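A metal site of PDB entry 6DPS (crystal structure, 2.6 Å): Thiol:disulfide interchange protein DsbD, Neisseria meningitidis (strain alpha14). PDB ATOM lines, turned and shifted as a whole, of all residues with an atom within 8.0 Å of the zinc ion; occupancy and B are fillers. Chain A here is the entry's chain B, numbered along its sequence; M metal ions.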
ATOM      1  N   GLY A  33       6.575 -10.169 -18.702  1.00  0.00           N
ATOM      2  CA  GLY A  33       7.794  -9.553 -19.163  1.00  0.00           C
ATOM      3  C   GLY A  33       7.711  -8.056 -19.366  1.00  0.00           C
ATOM      4  O   GLY A  33       8.647  -7.470 -19.906  1.00  0.00           O
ATOM      5  N   TYR A  34       6.610  -7.431 -18.946  1.00  0.00           N
ATOM      6  CA  TYR A  34       6.380  -5.990 -19.072  1.00  0.00           C
ATOM      7  C   TYR A  34       5.896  -5.420 -17.734  1.00  0.00           C
ATOM      8  O   TYR A  34       5.478  -6.159 -16.841  1.00  0.00           O
ATOM      9  CB  TYR A  34       5.371  -5.726 -20.218  1.00  0.00           C
ATOM     10  CG  TYR A  34       5.830  -6.250 -21.566  1.00  0.00           C
ATOM     11  CD1 TYR A  34       5.782  -7.622 -21.852  1.00  0.00           C
ATOM     12  CD2 TYR A  34       6.349  -5.386 -22.538  1.00  0.00           C
ATOM     13  CE1 TYR A  34       6.246  -8.102 -23.077  1.00  0.00           C
ATOM     14  CE2 TYR A  34       6.793  -5.858 -23.763  1.00  0.00           C
ATOM     15  CZ  TYR A  34       6.738  -7.225 -24.029  1.00  0.00           C
ATOM     16  OH  TYR A  34       7.200  -7.686 -25.259  1.00  0.00           O
ATOM     17  N   TYR A  35       5.978  -4.101 -17.583  1.00  0.00           N
ATOM     18  CA  TYR A  35       5.462  -3.474 -16.372  1.00  0.00           C
ATOM     19  C   TYR A  35       5.063  -2.048 -16.681  1.00  0.00           C
ATOM     20  O   TYR A  35       5.518  -1.476 -17.668  1.00  0.00           O
ATOM     21  CB  TYR A  35       6.465  -3.501 -15.230  1.00  0.00           C
ATOM     22  CG  TYR A  35       7.769  -2.781 -15.491  1.00  0.00           C
ATOM     23  CD1 TYR A  35       8.836  -3.445 -16.083  1.00  0.00           C
ATOM     24  CD2 TYR A  35       7.961  -1.453 -15.075  1.00  0.00           C
ATOM     25  CE1 TYR A  35      10.072  -2.802 -16.292  1.00  0.00           C
ATOM     26  CE2 TYR A  35       9.180  -0.793 -15.254  1.00  0.00           C
ATOM     27  CZ  TYR A  35      10.221  -1.471 -15.892  1.00  0.00           C
ATOM     28  OH  TYR A  35      11.404  -0.837 -16.112  1.00  0.00           O
ATOM     29  N   MET A  36       4.225  -1.473 -15.811  1.00  0.00           N
ATOM     30  CA  MET A  36       3.731  -0.111 -15.974  1.00  0.00           C
ATOM     31  C   MET A  36       4.163   0.776 -14.815  1.00  0.00           C
ATOM     32  O   MET A  36       4.242   0.335 -13.664  1.00  0.00           O
ATOM     33  CB  MET A  36       2.193  -0.068 -16.076  1.00  0.00           C
ATOM     34  CG  MET A  36       1.629  -0.850 -17.258  1.00  0.00           C
ATOM     35  SD  MET A  36      -0.182  -0.877 -17.325  1.00  0.00           S
ATOM     36  CE  MET A  36      -0.491   0.827 -17.797  1.00  0.00           C
ATOM     37  N   GLU A  60       4.143  -2.320  -6.709  1.00  0.00           N
ATOM     38  CA  GLU A  60       5.409  -2.756  -6.145  1.00  0.00           C
ATOM     39  C   GLU A  60       6.452  -1.669  -6.371  1.00  0.00           C
ATOM     40  O   GLU A  60       6.326  -0.832  -7.271  1.00  0.00           O
ATOM     41  CB  GLU A  60       5.885  -4.081  -6.766  1.00  0.00           C
ATOM     42  CG  GLU A  60       4.801  -5.128  -6.798  1.00  0.00           C
ATOM     43  CD  GLU A  60       5.132  -6.214  -7.750  1.00  0.00           C
ATOM     44  OE1 GLU A  60       6.099  -6.935  -7.475  1.00  0.00           O
ATOM     45  OE2 GLU A  60       4.427  -6.336  -8.785  1.00  0.00           O
ATOM     46  N   GLU A  61       7.480  -1.692  -5.536  1.00  0.00           N
ATOM     47  CA  GLU A  61       8.565  -0.744  -5.675  1.00  0.00           C
ATOM     48  C   GLU A  61       9.672  -1.335  -6.513  1.00  0.00           C
ATOM     49  O   GLU A  61       9.972  -2.531  -6.435  1.00  0.00           O
ATOM     50  CB  GLU A  61       9.087  -0.302  -4.308  1.00  0.00           C
ATOM     51  CG  GLU A  61       8.000   0.302  -3.466  1.00  0.00           C
ATOM     52  CD  GLU A  61       7.298   1.461  -4.151  1.00  0.00           C
ATOM     53  OE1 GLU A  61       8.010   2.429  -4.540  1.00  0.00           O
ATOM     54  OE2 GLU A  61       6.055   1.399  -4.294  1.00  0.00           O
ATOM     55  N   LYS A  62      10.263  -0.491  -7.354  1.00  0.00           N
ATOM     56  CA  LYS A  62      11.287  -0.925  -8.278  1.00  0.00           C
ATOM     57  C   LYS A  62      12.213   0.254  -8.503  1.00  0.00           C
ATOM     58  O   LYS A  62      11.796   1.405  -8.438  1.00  0.00           O
ATOM     59  CB  LYS A  62      10.634  -1.409  -9.594  1.00  0.00           C
ATOM     60  CG  LYS A  62      11.573  -1.444 -10.777  1.00  0.00           C
ATOM     61  CD  LYS A  62      10.849  -1.817 -12.043  1.00  0.00           C
ATOM     62  CE  LYS A  62      10.848  -3.306 -12.198  1.00  0.00           C
ATOM     63  NZ  LYS A  62      10.013  -3.711 -13.345  1.00  0.00           N
ATOM     64  N   ASP A  64      14.583   1.293 -11.656  1.00  0.00           N
ATOM     65  CA  ASP A  64      15.132   1.005 -12.977  1.00  0.00           C
ATOM     66  C   ASP A  64      15.978   2.176 -13.472  1.00  0.00           C
ATOM     67  O   ASP A  64      15.986   3.269 -12.892  1.00  0.00           O
ATOM     68  CB  ASP A  64      14.036   0.593 -13.973  1.00  0.00           C
ATOM     69  CG  ASP A  64      13.122   1.728 -14.393  1.00  0.00           C
ATOM     70  OD1 ASP A  64      13.438   2.919 -14.227  1.00  0.00           O
ATOM     71  OD2 ASP A  64      12.072   1.410 -14.981  1.00  0.00           O
ATOM     72  N   VAL A  72       5.483   0.401  -9.405  1.00  0.00           N
ATOM     73  CA  VAL A  72       5.200  -0.220 -10.679  1.00  0.00           C
ATOM     74  C   VAL A  72       4.167  -1.325 -10.524  1.00  0.00           C
ATOM     75  O   VAL A  72       3.854  -1.804  -9.436  1.00  0.00           O
ATOM     76  CB  VAL A  72       6.457  -0.779 -11.379  1.00  0.00           C
ATOM     77  CG1 VAL A  72       7.545   0.283 -11.446  1.00  0.00           C
ATOM     78  CG2 VAL A  72       6.950  -2.037 -10.711  1.00  0.00           C
ATOM     79  N   TYR A  73       3.646  -1.742 -11.678  1.00  0.00           N
ATOM     80  CA  TYR A  73       2.677  -2.823 -11.768  1.00  0.00           C
ATOM     81  C   TYR A  73       3.228  -3.913 -12.664  1.00  0.00           C
ATOM     82  O   TYR A  73       3.639  -3.646 -13.799  1.00  0.00           O
ATOM     83  CB  TYR A  73       1.346  -2.343 -12.335  1.00  0.00           C
ATOM     84  CG  TYR A  73       0.567  -1.469 -11.421  1.00  0.00           C
ATOM     85  CD1 TYR A  73       0.039  -1.969 -10.215  1.00  0.00           C
ATOM     86  CD2 TYR A  73       0.322  -0.138 -11.755  1.00  0.00           C
ATOM     87  CE1 TYR A  73      -0.728  -1.135  -9.375  1.00  0.00           C
ATOM     88  CE2 TYR A  73      -0.437   0.682 -10.933  1.00  0.00           C
ATOM     89  CZ  TYR A  73      -0.959   0.197  -9.753  1.00  0.00           C
ATOM     90  OH  TYR A  73      -1.695   1.061  -8.968  1.00  0.00           O
ATOM     91  N   HIS A  74       3.262  -5.131 -12.136  1.00  0.00           N
ATOM     92  CA  HIS A  74       3.348  -6.327 -12.940  1.00  0.00           C
ATOM     93  C   HIS A  74       1.960  -6.954 -12.998  1.00  0.00           C
ATOM     94  O   HIS A  74       1.155  -6.780 -12.082  1.00  0.00           O
ATOM     95  CB  HIS A  74       4.358  -7.339 -12.368  1.00  0.00           C
ATOM     96  CG  HIS A  74       5.754  -6.806 -12.159  1.00  0.00           C
ATOM     97  ND1 HIS A  74       6.241  -6.431 -10.915  1.00  0.00           N
ATOM     98  CD2 HIS A  74       6.792  -6.660 -13.018  1.00  0.00           C
ATOM     99  CE1 HIS A  74       7.507  -6.052 -11.032  1.00  0.00           C
ATOM    100  NE2 HIS A  74       7.862  -6.167 -12.293  1.00  0.00           N
ATOM    101  N   CYS A 100       7.073  -0.470 -19.782  1.00  0.00           N
ATOM    102  CA  CYS A 100       8.387  -0.874 -20.239  1.00  0.00           C
ATOM    103  C   CYS A 100       8.432  -2.381 -20.364  1.00  0.00           C
ATOM    104  O   CYS A 100       7.526  -3.103 -19.956  1.00  0.00           O
ATOM    105  CB  CYS A 100       9.479  -0.423 -19.254  1.00  0.00           C
ATOM    106  SG  CYS A 100       9.446   1.352 -18.871  1.00  0.00           S
ATOM    107  N   ALA A 101       9.527  -2.871 -20.904  1.00  0.00           N
ATOM    108  CA  ALA A 101       9.772  -4.289 -21.007  1.00  0.00           C
ATOM    109  C   ALA A 101      10.926  -4.650 -20.083  1.00  0.00           C
ATOM    110  O   ALA A 101      11.925  -3.912 -20.005  1.00  0.00           O
ATOM    111  CB  ALA A 101      10.066  -4.680 -22.454  1.00  0.00           C
ATOM    112  N   GLU A 102      10.797  -5.778 -19.391  1.00  0.00           N
ATOM    113  CA  GLU A 102      11.817  -6.208 -18.440  1.00  0.00           C
ATOM    114  C   GLU A 102      13.202  -6.312 -19.044  1.00  0.00           C
ATOM    115  O   GLU A 102      14.200  -6.164 -18.338  1.00  0.00           O
ATOM    116  CB  GLU A 102      11.449  -7.552 -17.802  1.00  0.00           C
ATOM    117  CG  GLU A 102      10.186  -7.494 -16.949  1.00  0.00           C
ATOM    118  CD  GLU A 102      10.325  -6.646 -15.668  1.00  0.00           C
ATOM    119  OE1 GLU A 102      11.371  -5.999 -15.444  1.00  0.00           O
ATOM    120  OE2 GLU A 102       9.365  -6.608 -14.892  1.00  0.00           O
HETATM  121 ZN    ZN M   1       9.708  -5.826 -13.084  1.00  0.00          ZN
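Merely in contact with the zinc ion: Tyr 35.
Of the 14 residues printed, 4 come within 4 Å of the zinc ion.
The nearest printed residue that does not touch the zinc ion is Val 72 (5.3 Å).
The backbone carbonyl oxygen (O) of Gly 33 sits at hydrogen-bond distance from the backbone NH (N) of Glu 102 (2.8 Å).
A ring nitrogen (ND1) of His 74 sits at hydrogen-bond distance from the side-chain carboxylate (OE2) of Glu 60 (2.8 Å).
The backbone carbonyl oxygen (O) of Tyr 35 lies within hydrogen-bond range of the backbone NH (N) of Cys 100.
The side-chain carboxylate (OD2) of Asp 64 sits at hydrogen-bond distance from the side-chain hydroxyl (OH) of Tyr 35, 2.6 Å away.
The zinc ion is bound by OE2 of Glu 102 (2.0 Å).
A ring nitrogen (NE2) of His 74 is bound to the zinc ion.
The zinc ion is bound by NZ of Lys 62 (2.2 Å).
The zinc ion has three donor atoms within binding distance.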
